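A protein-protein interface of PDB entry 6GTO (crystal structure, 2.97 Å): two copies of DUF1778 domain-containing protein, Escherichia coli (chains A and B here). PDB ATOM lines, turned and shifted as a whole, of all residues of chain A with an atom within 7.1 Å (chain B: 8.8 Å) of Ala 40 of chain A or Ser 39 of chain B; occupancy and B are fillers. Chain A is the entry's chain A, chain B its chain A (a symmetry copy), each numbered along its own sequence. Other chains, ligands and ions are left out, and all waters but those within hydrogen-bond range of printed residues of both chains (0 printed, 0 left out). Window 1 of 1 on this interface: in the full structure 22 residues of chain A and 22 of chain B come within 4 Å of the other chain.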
ATOM      1  N   ILE A  21     -24.758 -29.137  21.206  1.00  0.00           N
ATOM      2  CA  ILE A  21     -24.136 -27.847  21.513  1.00  0.00           C
ATOM      3  C   ILE A  21     -25.056 -26.693  21.083  1.00  0.00           C
ATOM      4  O   ILE A  21     -25.285 -25.798  21.890  1.00  0.00           O
ATOM      5  CB  ILE A  21     -22.680 -27.720  20.979  1.00  0.00           C
ATOM      6  CG1 ILE A  21     -21.845 -28.947  21.398  1.00  0.00           C
ATOM      7  CG2 ILE A  21     -22.022 -26.419  21.468  1.00  0.00           C
ATOM      8  CD1 ILE A  21     -20.421 -28.991  20.918  1.00  0.00           C
ATOM      9  N   GLN A  34     -19.826 -18.698  22.650  1.00  0.00           N
ATOM     10  CA  GLN A  34     -19.728 -18.311  24.056  1.00  0.00           C
ATOM     11  C   GLN A  34     -19.928 -19.509  24.961  1.00  0.00           C
ATOM     12  O   GLN A  34     -19.240 -19.612  25.971  1.00  0.00           O
ATOM     13  CB  GLN A  34     -20.692 -17.175  24.420  1.00  0.00           C
ATOM     14  CG  GLN A  34     -20.347 -16.448  25.734  1.00  0.00           C
ATOM     15  CD  GLN A  34     -18.901 -16.000  25.839  1.00  0.00           C
ATOM     16  OE1 GLN A  34     -18.182 -16.375  26.766  1.00  0.00           O
ATOM     17  NE2 GLN A  34     -18.435 -15.190  24.894  1.00  0.00           N
ATOM     18  N   PHE A  35     -20.837 -20.428  24.587  1.00  0.00           N
ATOM     19  CA  PHE A  35     -21.091 -21.645  25.343  1.00  0.00           C
ATOM     20  C   PHE A  35     -19.842 -22.500  25.375  1.00  0.00           C
ATOM     21  O   PHE A  35     -19.455 -22.937  26.453  1.00  0.00           O
ATOM     22  CB  PHE A  35     -22.243 -22.434  24.730  1.00  0.00           C
ATOM     23  CG  PHE A  35     -22.547 -23.718  25.457  1.00  0.00           C
ATOM     24  CD1 PHE A  35     -23.316 -23.714  26.614  1.00  0.00           C
ATOM     25  CD2 PHE A  35     -22.079 -24.936  24.977  1.00  0.00           C
ATOM     26  CE1 PHE A  35     -23.592 -24.902  27.288  1.00  0.00           C
ATOM     27  CE2 PHE A  35     -22.363 -26.127  25.649  1.00  0.00           C
ATOM     28  CZ  PHE A  35     -23.115 -26.103  26.800  1.00  0.00           C
ATOM     29  N   MET A  36     -19.215 -22.729  24.201  1.00  0.00           N
ATOM     30  CA  MET A  36     -17.992 -23.516  24.025  1.00  0.00           C
ATOM     31  C   MET A  36     -16.840 -22.990  24.871  1.00  0.00           C
ATOM     32  O   MET A  36     -16.181 -23.784  25.537  1.00  0.00           O
ATOM     33  CB  MET A  36     -17.574 -23.544  22.557  1.00  0.00           C
ATOM     34  CG  MET A  36     -18.301 -24.582  21.721  1.00  0.00           C
ATOM     35  SD  MET A  36     -17.605 -24.726  20.039  1.00  0.00           S
ATOM     36  CE  MET A  36     -15.742 -24.913  20.450  1.00  0.00           C
ATOM     37  N   LEU A  37     -16.602 -21.656  24.859  1.00  0.00           N
ATOM     38  CA  LEU A  37     -15.543 -21.012  25.640  1.00  0.00           C
ATOM     39  C   LEU A  37     -15.857 -21.181  27.098  1.00  0.00           C
ATOM     40  O   LEU A  37     -15.065 -21.785  27.796  1.00  0.00           O
ATOM     41  CB  LEU A  37     -15.398 -19.523  25.304  1.00  0.00           C
ATOM     42  CG  LEU A  37     -14.938 -19.161  23.900  1.00  0.00           C
ATOM     43  CD1 LEU A  37     -14.931 -17.673  23.720  1.00  0.00           C
ATOM     44  CD2 LEU A  37     -13.554 -19.679  23.625  1.00  0.00           C
ATOM     45  N   ASN A  38     -17.050 -20.747  27.539  1.00  0.00           N
ATOM     46  CA  ASN A  38     -17.524 -20.877  28.919  1.00  0.00           C
ATOM     47  C   ASN A  38     -17.364 -22.289  29.483  1.00  0.00           C
ATOM     48  O   ASN A  38     -16.746 -22.439  30.540  1.00  0.00           O
ATOM     49  CB  ASN A  38     -18.968 -20.376  29.069  1.00  0.00           C
ATOM     50  CG  ASN A  38     -19.097 -18.871  29.144  1.00  0.00           C
ATOM     51  OD1 ASN A  38     -20.180 -18.342  29.411  1.00  0.00           O
ATOM     52  ND2 ASN A  38     -18.000 -18.140  28.926  1.00  0.00           N
ATOM     53  N   SER A  39     -17.869 -23.320  28.771  1.00  0.00           N
ATOM     54  CA  SER A  39     -17.726 -24.708  29.213  1.00  0.00           C
ATOM     55  C   SER A  39     -16.230 -25.154  29.268  1.00  0.00           C
ATOM     56  O   SER A  39     -15.793 -25.677  30.297  1.00  0.00           O
ATOM     57  CB  SER A  39     -18.612 -25.650  28.400  1.00  0.00           C
ATOM     58  OG  SER A  39     -18.579 -25.415  27.006  1.00  0.00           O
ATOM     59  N   ALA A  40     -15.431 -24.837  28.235  1.00  0.00           N
ATOM     60  CA  ALA A  40     -13.999 -25.132  28.232  1.00  0.00           C
ATOM     61  C   ALA A  40     -13.291 -24.464  29.420  1.00  0.00           C
ATOM     62  O   ALA A  40     -12.458 -25.083  30.070  1.00  0.00           O
ATOM     63  CB  ALA A  40     -13.381 -24.652  26.938  1.00  0.00           C
ATOM     64  N   SER A  41     -13.653 -23.209  29.708  1.00  0.00           N
ATOM     65  CA  SER A  41     -13.123 -22.380  30.784  1.00  0.00           C
ATOM     66  C   SER A  41     -13.401 -22.972  32.157  1.00  0.00           C
ATOM     67  O   SER A  41     -12.504 -22.978  32.988  1.00  0.00           O
ATOM     68  CB  SER A  41     -13.698 -20.968  30.682  1.00  0.00           C
ATOM     69  OG  SER A  41     -13.487 -20.190  31.848  1.00  0.00           O
ATOM     70  N   GLN A  42     -14.638 -23.448  32.401  1.00  0.00           N
ATOM     71  CA  GLN A  42     -15.019 -24.005  33.697  1.00  0.00           C
ATOM     72  C   GLN A  42     -14.610 -25.456  33.855  1.00  0.00           C
ATOM     73  O   GLN A  42     -14.316 -25.867  34.982  1.00  0.00           O
ATOM     74  CB  GLN A  42     -16.503 -23.791  34.028  1.00  0.00           C
ATOM     75  CG  GLN A  42     -17.502 -24.425  33.082  1.00  0.00           C
ATOM     76  CD  GLN A  42     -18.898 -23.980  33.435  1.00  0.00           C
ATOM     77  OE1 GLN A  42     -19.541 -24.540  34.334  1.00  0.00           O
ATOM     78  NE2 GLN A  42     -19.393 -22.958  32.743  1.00  0.00           N
ATOM     79  N   ARG A  43     -14.549 -26.226  32.747  1.00  0.00           N
ATOM     80  CA  ARG A  43     -14.095 -27.614  32.814  1.00  0.00           C
ATOM     81  C   ARG A  43     -12.579 -27.639  33.020  1.00  0.00           C
ATOM     82  O   ARG A  43     -12.084 -28.569  33.645  1.00  0.00           O
ATOM     83  CB  ARG A  43     -14.534 -28.408  31.586  1.00  0.00           C
ATOM     84  CG  ARG A  43     -13.831 -29.730  31.401  1.00  0.00           C
ATOM     85  CD  ARG A  43     -14.491 -30.920  32.083  1.00  0.00           C
ATOM     86  NE  ARG A  43     -13.612 -32.103  32.089  1.00  0.00           N
ATOM     87  CZ  ARG A  43     -13.127 -32.716  31.001  1.00  0.00           C
ATOM     88  NH1 ARG A  43     -13.416 -32.261  29.782  1.00  0.00           N
ATOM     89  NH2 ARG A  43     -12.340 -33.779  31.128  1.00  0.00           N
ATOM     90  N   ALA A  44     -11.852 -26.589  32.548  1.00  0.00           N
ATOM     91  CA  ALA A  44     -10.412 -26.425  32.745  1.00  0.00           C
ATOM     92  C   ALA A  44     -10.126 -26.334  34.232  1.00  0.00           C
ATOM     93  O   ALA A  44      -9.229 -27.011  34.702  1.00  0.00           O
ATOM     94  CB  ALA A  44      -9.914 -25.173  32.047  1.00  0.00           C
ATOM     95  N   ALA A  45     -10.945 -25.565  34.977  1.00  0.00           N
ATOM     96  CA  ALA A  45     -10.879 -25.399  36.428  1.00  0.00           C
ATOM     97  C   ALA A  45     -11.034 -26.739  37.155  1.00  0.00           C
ATOM     98  O   ALA A  45     -10.190 -27.090  37.981  1.00  0.00           O
ATOM     99  CB  ALA A  45     -11.960 -24.434  36.881  1.00  0.00           C
ATOM    100  N   LEU B  13     -12.681 -13.921  26.616  1.00  0.00           N
ATOM    101  CA  LEU B  13     -11.839 -14.848  27.374  1.00  0.00           C
ATOM    102  C   LEU B  13     -10.710 -14.123  28.112  1.00  0.00           C
ATOM    103  O   LEU B  13      -9.987 -13.331  27.516  1.00  0.00           O
ATOM    104  CB  LEU B  13     -11.255 -15.917  26.453  1.00  0.00           C
ATOM    105  CG  LEU B  13     -11.158 -17.328  27.033  1.00  0.00           C
ATOM    106  N   ASP B  17      -7.671 -17.188  32.016  1.00  0.00           N
ATOM    107  CA  ASP B  17      -8.582 -18.286  31.698  1.00  0.00           C
ATOM    108  C   ASP B  17      -8.029 -19.050  30.492  1.00  0.00           C
ATOM    109  O   ASP B  17      -8.234 -20.256  30.379  1.00  0.00           O
ATOM    110  CB  ASP B  17      -9.999 -17.754  31.402  1.00  0.00           C
ATOM    111  CG  ASP B  17     -10.905 -17.587  32.621  1.00  0.00           C
ATOM    112  OD1 ASP B  17     -10.963 -18.526  33.461  1.00  0.00           O
ATOM    113  OD2 ASP B  17     -11.586 -16.536  32.719  1.00  0.00           O
ATOM    114  N   LYS B  18      -7.316 -18.335  29.595  1.00  0.00           N
ATOM    115  CA  LYS B  18      -6.663 -18.895  28.409  1.00  0.00           C
ATOM    116  C   LYS B  18      -5.526 -19.789  28.889  1.00  0.00           C
ATOM    117  O   LYS B  18      -5.236 -20.799  28.264  1.00  0.00           O
ATOM    118  CB  LYS B  18      -6.120 -17.774  27.493  1.00  0.00           C
ATOM    119  CG  LYS B  18      -7.158 -17.089  26.606  1.00  0.00           C
ATOM    120  N   MET B  20      -5.492 -21.412  31.982  1.00  0.00           N
ATOM    121  CA  MET B  20      -6.175 -22.567  32.579  1.00  0.00           C
ATOM    122  C   MET B  20      -6.483 -23.634  31.532  1.00  0.00           C
ATOM    123  O   MET B  20      -6.276 -24.811  31.794  1.00  0.00           O
ATOM    124  CB  MET B  20      -7.502 -22.134  33.195  1.00  0.00           C
ATOM    125  CG  MET B  20      -7.408 -21.621  34.585  1.00  0.00           C
ATOM    126  SD  MET B  20      -9.101 -21.424  35.218  1.00  0.00           S
ATOM    127  CE  MET B  20      -8.718 -20.668  36.843  1.00  0.00           C
ATOM    128  N   ILE B  21      -6.993 -23.217  30.353  1.00  0.00           N
ATOM    129  CA  ILE B  21      -7.334 -24.104  29.238  1.00  0.00           C
ATOM    130  C   ILE B  21      -6.064 -24.758  28.668  1.00  0.00           C
ATOM    131  O   ILE B  21      -6.060 -25.974  28.504  1.00  0.00           O
ATOM    132  CB  ILE B  21      -8.228 -23.425  28.159  1.00  0.00           C
ATOM    133  CG1 ILE B  21      -9.439 -22.738  28.821  1.00  0.00           C
ATOM    134  CG2 ILE B  21      -8.687 -24.443  27.103  1.00  0.00           C
ATOM    135  CD1 ILE B  21     -10.378 -21.998  27.909  1.00  0.00           C
ATOM    136  N   GLU B  22      -4.983 -23.989  28.437  1.00  0.00           N
ATOM    137  CA  GLU B  22      -3.712 -24.538  27.946  1.00  0.00           C
ATOM    138  C   GLU B  22      -3.142 -25.586  28.929  1.00  0.00           C
ATOM    139  O   GLU B  22      -2.677 -26.648  28.509  1.00  0.00           O
ATOM    140  CB  GLU B  22      -2.693 -23.418  27.754  1.00  0.00           C
ATOM    141  CG  GLU B  22      -2.981 -22.501  26.582  1.00  0.00           C
ATOM    142  CD  GLU B  22      -2.059 -21.299  26.465  1.00  0.00           C
ATOM    143  OE1 GLU B  22      -1.819 -20.614  27.486  1.00  0.00           O
ATOM    144  OE2 GLU B  22      -1.590 -21.036  25.337  1.00  0.00           O
ATOM    145  N   ALA B  24      -4.944 -27.267  31.472  1.00  0.00           N
ATOM    146  CA  ALA B  24      -5.865 -28.395  31.596  1.00  0.00           C
ATOM    147  C   ALA B  24      -5.836 -29.293  30.381  1.00  0.00           C
ATOM    148  O   ALA B  24      -5.996 -30.505  30.531  1.00  0.00           O
ATOM    149  CB  ALA B  24      -7.264 -27.906  31.848  1.00  0.00           C
ATOM    150  N   ALA B  25      -5.594 -28.722  29.180  1.00  0.00           N
ATOM    151  CA  ALA B  25      -5.482 -29.521  27.961  1.00  0.00           C
ATOM    152  C   ALA B  25      -4.211 -30.368  28.069  1.00  0.00           C
ATOM    153  O   ALA B  25      -4.247 -31.561  27.768  1.00  0.00           O
ATOM    154  CB  ALA B  25      -5.432 -28.631  26.729  1.00  0.00           C
ATOM    155  N   SER B  28      -4.863 -33.294  30.508  1.00  0.00           N
ATOM    156  CA  SER B  28      -5.746 -34.215  29.792  1.00  0.00           C
ATOM    157  C   SER B  28      -5.062 -34.893  28.604  1.00  0.00           C
ATOM    158  O   SER B  28      -5.625 -35.830  28.039  1.00  0.00           O
ATOM    159  CB  SER B  28      -6.971 -33.461  29.300  1.00  0.00           C
ATOM    160  OG  SER B  28      -7.563 -32.730  30.359  1.00  0.00           O
ATOM    161  N   GLN B  30      -4.402 -33.658  25.543  1.00  0.00           N
ATOM    162  CA  GLN B  30      -5.185 -33.276  24.358  1.00  0.00           C
ATOM    163  C   GLN B  30      -4.753 -31.877  23.881  1.00  0.00           C
ATOM    164  O   GLN B  30      -4.136 -31.127  24.647  1.00  0.00           O
ATOM    165  CB  GLN B  30      -6.678 -33.167  24.699  1.00  0.00           C
ATOM    166  CG  GLN B  30      -7.306 -34.339  25.398  1.00  0.00           C
ATOM    167  CD  GLN B  30      -8.787 -34.114  25.419  1.00  0.00           C
ATOM    168  OE1 GLN B  30      -9.324 -33.387  26.263  1.00  0.00           O
ATOM    169  NE2 GLN B  30      -9.477 -34.710  24.462  1.00  0.00           N
ATOM    170  N   SER B  31      -5.139 -31.500  22.644  1.00  0.00           N
ATOM    171  CA  SER B  31      -4.858 -30.162  22.129  1.00  0.00           C
ATOM    172  C   SER B  31      -5.883 -29.206  22.744  1.00  0.00           C
ATOM    173  O   SER B  31      -6.942 -29.664  23.188  1.00  0.00           O
ATOM    174  CB  SER B  31      -4.939 -30.139  20.605  1.00  0.00           C
ATOM    175  OG  SER B  31      -6.217 -30.522  20.127  1.00  0.00           O
ATOM    176  N   VAL B  32      -5.577 -27.891  22.789  1.00  0.00           N
ATOM    177  CA  VAL B  32      -6.479 -26.878  23.359  1.00  0.00           C
ATOM    178  C   VAL B  32      -7.828 -26.906  22.628  1.00  0.00           C
ATOM    179  O   VAL B  32      -8.871 -26.761  23.267  1.00  0.00           O
ATOM    180  CB  VAL B  32      -5.838 -25.469  23.397  1.00  0.00           C
ATOM    181  CG1 VAL B  32      -6.824 -24.416  23.861  1.00  0.00           C
ATOM    182  CG2 VAL B  32      -4.612 -25.450  24.295  1.00  0.00           C
ATOM    183  N   SER B  33      -7.804 -27.170  21.305  1.00  0.00           N
ATOM    184  CA  SER B  33      -8.998 -27.247  20.460  1.00  0.00           C
ATOM    185  C   SER B  33      -9.803 -28.496  20.752  1.00  0.00           C
ATOM    186  O   SER B  33     -11.026 -28.398  20.861  1.00  0.00           O
ATOM    187  CB  SER B  33      -8.620 -27.190  18.985  1.00  0.00           C
ATOM    188  N   GLN B  34      -9.135 -29.661  20.905  1.00  0.00           N
ATOM    189  CA  GLN B  34      -9.833 -30.906  21.219  1.00  0.00           C
ATOM    190  C   GLN B  34     -10.433 -30.854  22.610  1.00  0.00           C
ATOM    191  O   GLN B  34     -11.538 -31.350  22.798  1.00  0.00           O
ATOM    192  CB  GLN B  34      -8.936 -32.140  21.050  1.00  0.00           C
ATOM    193  CG  GLN B  34      -9.704 -33.471  20.948  1.00  0.00           C
ATOM    194  CD  GLN B  34     -10.833 -33.467  19.935  1.00  0.00           C
ATOM    195  OE1 GLN B  34     -11.991 -33.720  20.267  1.00  0.00           O
ATOM    196  NE2 GLN B  34     -10.530 -33.175  18.673  1.00  0.00           N
ATOM    197  N   PHE B  35      -9.728 -30.227  23.569  1.00  0.00           N
ATOM    198  CA  PHE B  35     -10.213 -30.068  24.931  1.00  0.00           C
ATOM    199  C   PHE B  35     -11.474 -29.229  24.934  1.00  0.00           C
ATOM    200  O   PHE B  35     -12.452 -29.638  25.550  1.00  0.00           O
ATOM    201  CB  PHE B  35      -9.153 -29.411  25.810  1.00  0.00           C
ATOM    202  CG  PHE B  35      -9.598 -29.201  27.234  1.00  0.00           C
ATOM    203  CD1 PHE B  35      -9.553 -30.241  28.154  1.00  0.00           C
ATOM    204  CD2 PHE B  35     -10.049 -27.957  27.663  1.00  0.00           C
ATOM    205  CE1 PHE B  35      -9.971 -30.046  29.469  1.00  0.00           C
ATOM    206  CE2 PHE B  35     -10.460 -27.760  28.983  1.00  0.00           C
ATOM    207  CZ  PHE B  35     -10.420 -28.804  29.877  1.00  0.00           C
ATOM    208  N   MET B  36     -11.450 -28.070  24.242  1.00  0.00           N
ATOM    209  CA  MET B  36     -12.566 -27.130  24.112  1.00  0.00           C
ATOM    210  C   MET B  36     -13.812 -27.789  23.532  1.00  0.00           C
ATOM    211  O   MET B  36     -14.893 -27.601  24.081  1.00  0.00           O
ATOM    212  CB  MET B  36     -12.171 -25.937  23.246  1.00  0.00           C
ATOM    213  CG  MET B  36     -11.411 -24.852  23.988  1.00  0.00           C
ATOM    214  SD  MET B  36     -11.165 -23.359  22.966  1.00  0.00           S
ATOM    215  CE  MET B  36     -12.954 -23.066  22.344  1.00  0.00           C
ATOM    216  N   LEU B  37     -13.662 -28.569  22.434  1.00  0.00           N
ATOM    217  CA  LEU B  37     -14.767 -29.279  21.785  1.00  0.00           C
ATOM    218  C   LEU B  37     -15.293 -30.313  22.737  1.00  0.00           C
ATOM    219  O   LEU B  37     -16.453 -30.235  23.096  1.00  0.00           O
ATOM    220  CB  LEU B  37     -14.337 -29.945  20.472  1.00  0.00           C
ATOM    221  CG  LEU B  37     -13.910 -29.036  19.330  1.00  0.00           C
ATOM    222  CD1 LEU B  37     -13.447 -29.851  18.161  1.00  0.00           C
ATOM    223  CD2 LEU B  37     -15.040 -28.155  18.877  1.00  0.00           C
ATOM    224  N   ASN B  38     -14.426 -31.213  23.231  1.00  0.00           N
ATOM    225  CA  ASN B  38     -14.771 -32.255  24.200  1.00  0.00           C
ATOM    226  C   ASN B  38     -15.548 -31.727  25.407  1.00  0.00           C
ATOM    227  O   ASN B  38     -16.632 -32.244  25.687  1.00  0.00           O
ATOM    228  CB  ASN B  38     -13.532 -33.050  24.639  1.00  0.00           C
ATOM    229  CG  ASN B  38     -13.082 -34.095  23.643  1.00  0.00           C
ATOM    230  OD1 ASN B  38     -12.192 -34.901  23.931  1.00  0.00           O
ATOM    231  ND2 ASN B  38     -13.688 -34.124  22.453  1.00  0.00           N
ATOM    232  N   SER B  39     -15.032 -30.680  26.088  1.00  0.00           N
ATOM    233  CA  SER B  39     -15.726 -30.082  27.228  1.00  0.00           C
ATOM    234  C   SER B  39     -17.099 -29.458  26.818  1.00  0.00           C
ATOM    235  O   SER B  39     -18.115 -29.764  27.448  1.00  0.00           O
ATOM    236  CB  SER B  39     -14.824 -29.115  27.991  1.00  0.00           C
ATOM    237  OG  SER B  39     -14.082 -28.241  27.163  1.00  0.00           O
ATOM    238  N   ALA B  40     -17.150 -28.705  25.705  1.00  0.00           N
ATOM    239  CA  ALA B  40     -18.402 -28.152  25.190  1.00  0.00           C
ATOM    240  C   ALA B  40     -19.419 -29.262  24.888  1.00  0.00           C
ATOM    241  O   ALA B  40     -20.591 -29.131  25.215  1.00  0.00           O
ATOM    242  CB  ALA B  40     -18.130 -27.357  23.932  1.00  0.00           C
ATOM    243  N   SER B  41     -18.949 -30.362  24.292  1.00  0.00           N
ATOM    244  CA  SER B  41     -19.722 -31.540  23.913  1.00  0.00           C
ATOM    245  C   SER B  41     -20.341 -32.233  25.116  1.00  0.00           C
ATOM    246  O   SER B  41     -21.505 -32.607  25.046  1.00  0.00           O
ATOM    247  CB  SER B  41     -18.839 -32.510  23.130  1.00  0.00           C
ATOM    248  OG  SER B  41     -19.408 -33.801  22.991  1.00  0.00           O
ATOM    249  N   GLN B  42     -19.569 -32.422  26.204  1.00  0.00           N
ATOM    250  CA  GLN B  42     -20.056 -33.108  27.398  1.00  0.00           C
ATOM    251  C   GLN B  42     -20.841 -32.196  28.320  1.00  0.00           C
ATOM    252  O   GLN B  42     -21.761 -32.680  28.987  1.00  0.00           O
ATOM    253  CB  GLN B  42     -18.949 -33.862  28.149  1.00  0.00           C
ATOM    254  CG  GLN B  42     -17.807 -33.023  28.685  1.00  0.00           C
ATOM    255  CD  GLN B  42     -16.726 -33.918  29.233  1.00  0.00           C
ATOM    256  OE1 GLN B  42     -16.796 -34.379  30.381  1.00  0.00           O
ATOM    257  NE2 GLN B  42     -15.706 -34.190  28.422  1.00  0.00           N
ATOM    258  N   ARG B  43     -20.523 -30.883  28.341  1.00  0.00           N
ATOM    259  CA  ARG B  43     -21.283 -29.933  29.151  1.00  0.00           C
ATOM    260  C   ARG B  43     -22.642 -29.682  28.492  1.00  0.00           C
ATOM    261  O   ARG B  43     -23.603 -29.420  29.206  1.00  0.00           O
ATOM    262  CB  ARG B  43     -20.499 -28.645  29.388  1.00  0.00           C
ATOM    263  CG  ARG B  43     -21.319 -27.490  29.908  1.00  0.00           C
ATOM    264  CD  ARG B  43     -21.425 -27.397  31.425  1.00  0.00           C
ATOM    265  NE  ARG B  43     -22.451 -26.424  31.842  1.00  0.00           N
ATOM    266  CZ  ARG B  43     -22.453 -25.119  31.542  1.00  0.00           C
ATOM    267  NH1 ARG B  43     -21.479 -24.594  30.798  1.00  0.00           N
ATOM    268  NH2 ARG B  43     -23.434 -24.334  31.974  1.00  0.00           N
ATOM    269  N   ALA B  44     -22.733 -29.823  27.141  1.00  0.00           N
ATOM    270  CA  ALA B  44     -23.977 -29.705  26.380  1.00  0.00           C
ATOM    271  C   ALA B  44     -24.945 -30.773  26.851  1.00  0.00           C
ATOM    272  O   ALA B  44     -26.094 -30.457  27.105  1.00  0.00           O
ATOM    273  CB  ALA B  44     -23.714 -29.867  24.895  1.00  0.00           C
ATOM    274  N   ALA B  45     -24.454 -32.012  27.050  1.00  0.00           N
ATOM    275  CA  ALA B  45     -25.205 -33.158  27.561  1.00  0.00           C
ATOM    276  C   ALA B  45     -25.788 -32.874  28.951  1.00  0.00           C
ATOM    277  O   ALA B  45     -26.992 -33.038  29.156  1.00  0.00           O
ATOM    278  CB  ALA B  45     -24.302 -34.377  27.617  1.00  0.00           C
ATOM    279  N   GLU B  46     -24.932 -32.421  29.887  1.00  0.00           N
ATOM    280  CA  GLU B  46     -25.308 -32.071  31.265  1.00  0.00           C
ATOM    281  C   GLU B  46     -26.485 -31.093  31.281  1.00  0.00           C
ATOM    282  O   GLU B  46     -27.432 -31.317  32.023  1.00  0.00           O
ATOM    283  CB  GLU B  46     -24.118 -31.436  32.025  1.00  0.00           C
ATOM    284  CG  GLU B  46     -22.934 -32.351  32.312  1.00  0.00           C
ATOM    285  CD  GLU B  46     -21.645 -31.657  32.734  1.00  0.00           C
ATOM    286  OE1 GLU B  46     -21.716 -30.518  33.253  1.00  0.00           O
ATOM    287  OE2 GLU B  46     -20.559 -32.258  32.545  1.00  0.00           O
ATOM    288  N   VAL B  47     -26.409 -30.026  30.454  1.00  0.00           N
ATOM    289  CA  VAL B  47     -27.357 -28.923  30.301  1.00  0.00           C
ATOM    290  C   VAL B  47     -28.692 -29.402  29.763  1.00  0.00           C
ATOM    291  O   VAL B  47     -29.731 -28.946  30.241  1.00  0.00           O
ATOM    292  CB  VAL B  47     -26.738 -27.809  29.423  1.00  0.00           C
ATOM    293  CG1 VAL B  47     -27.775 -26.798  28.976  1.00  0.00           C
ATOM    294  CG2 VAL B  47     -25.608 -27.105  30.147  1.00  0.00           C
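OG of Ser 41 of chain A is in hydrogen-bond range of OD1 of Asp 17 of chain B, at 3.4 Å.
NE2 of Gln 42 of chain A lies close to NH1 of Arg 43 of chain B, at 3.3 Å.
The side-chain amide nitrogen (NE2) of Gln 42 of chain B sits close to the guanidinium group (NH1) of Arg 43 of chain A.
O of Met 36 of chain B sits at hydrogen-bond distance from OG of Ser 39 of chain B (3.3 Å).
The side-chain hydroxyl (OG) of Ser 39 of chain A is in hydrogen-bond range of the backbone carbonyl oxygen (O) of Met 36 of chain A, at 3.3 Å.
The side-chain amide nitrogen (NE2) of Gln 42 of chain B lies close to the backbone carbonyl oxygen (O) of Asn 38 of chain B (3.5 Å).
The backbone carbonyl oxygen (O) of Asn 38 of chain A lies close to the side-chain amide nitrogen (NE2) of Gln 42 of chain A (3.5 Å).
The backbone carbonyl oxygen of Phe 35 of chain A sits at hydrogen-bond distance from the side-chain hydroxyl of Ser 39 of chain A (2.7 Å).
O of Ala 24 of chain B lies within hydrogen-bond range of OG of Ser 28 of chain B.
Among the printed residues, merely in contact across the chains: Ala 40 of chain A with Ser 39 of chain B (3.3 Å), Ser 39 of chain A with Ala 40 of chain B (3.3 Å), Ala 40 of chain A with Phe 35 of chain B (3.5 Å), Phe 35 of chain A with Ala 40 of chain B (3.5 Å), Met 36 of chain A with Ala 40 of chain B (3.6 Å), Ala 40 of chain A with Met 36 of chain B (3.6 Å), Ala 44 of chain A with Ala 24 of chain B (3.6 Å), Ser 39 of chain A with Arg 43 of chain B (3.6 Å), Arg 43 of chain A with Ser 39 of chain B (3.6 Å), Ala 44 of chain A with Met 20 of chain B (3.7 Å), Leu 37 of chain A with Met 36 of chain B (3.7 Å), Met 36 of chain A with Leu 37 of chain B (3.7 Å), Ala 44 of chain A with Phe 35 of chain B (3.7 Å), Phe 35 of chain A with Ala 44 of chain B (3.7 Å), Met 36 of chain A with Met 36 of chain B (3.8 Å), Phe 35 of chain A with Arg 43 of chain B (3.8 Å), Arg 43 of chain A with Phe 35 of chain B (3.8 Å), Ala 44 of chain A with Ile 21 of chain B (3.9 Å), Ile 21 of chain A with Ala 44 of chain B (3.9 Å), Ser 41 of chain A with Ile 21 of chain B (3.9 Å) and Ile 21 of chain A with Ser 41 of chain B (3.9 Å).
Printed residues of chain B within 4 Å of Ile 21 of chain A: Ser 41 and Ala 44.
Gln 34 of chain A touches none of the printed residues of chain B.
Printed residues of chain B within 4 Å of Met 36 of chain A: Met 36, Leu 37 and Ala 40.
Ala 40 of chain A touches just these residues of chain B: Phe 35, Met 36 and Ser 39.
Glu 22 of chain B touches none of the printed residues of chain A.
Of the printed residues of chain A, Phe 35 of chain B touches Ala 40 (3.5 Å), Arg 43 (3.8 Å) and Ala 44 (3.7 Å).
Printed residues of chain A within 4 Å of Met 36 of chain B: Met 36, Leu 37 and Ala 40.
Of the printed residues of chain A, Ser 39 of chain B touches Ala 40 and Arg 43.
The nearest residue of chain A that does not touch Ser 39 of chain B is Ser 39 of chain A (4.3 Å).
The nearest printed residue of chain B that does not touch Ser 41 of chain A is Met 20 of chain B (4.4 Å).
Hydrophobic or aromatic side chains of chain A that line the printed part of chain B: Ile 21, Phe 35, Met 36, Leu 37, Ala 40 and Ala 44.
Along chain A the printed residues that touch a printed residue of chain B span positions 21 to 44.
Among the printed residues, 24 pairs touch across the chains.
Among the printed residues, no Asp or Glu carboxylate lies within 4 Å of a Lys or Arg side-chain nitrogen of the other chain.
Ile 21 of chain A touches Ser 41 of chain B, and with the chains exchanged Ser 41 of chain A touches Ile 21 of chain B.
Met 36 of chain A touches Ala 40 of chain B, and with the chains exchanged Ala 40 of chain A touches Met 36 of chain B.
Ser 39 of chain A touches Arg 43 of chain B, and with the chains exchanged Arg 43 of chain A touches Ser 39 of chain B.
Gln 42 of chain A touches Arg 43 of chain B, and with the chains exchanged Arg 43 of chain A touches Gln 42 of chain B.
13 positions are printed for both chains.
Of the 24 pairs that touch across the chains among the printed residues, 21 have their exchanged pair printed and touching as well.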
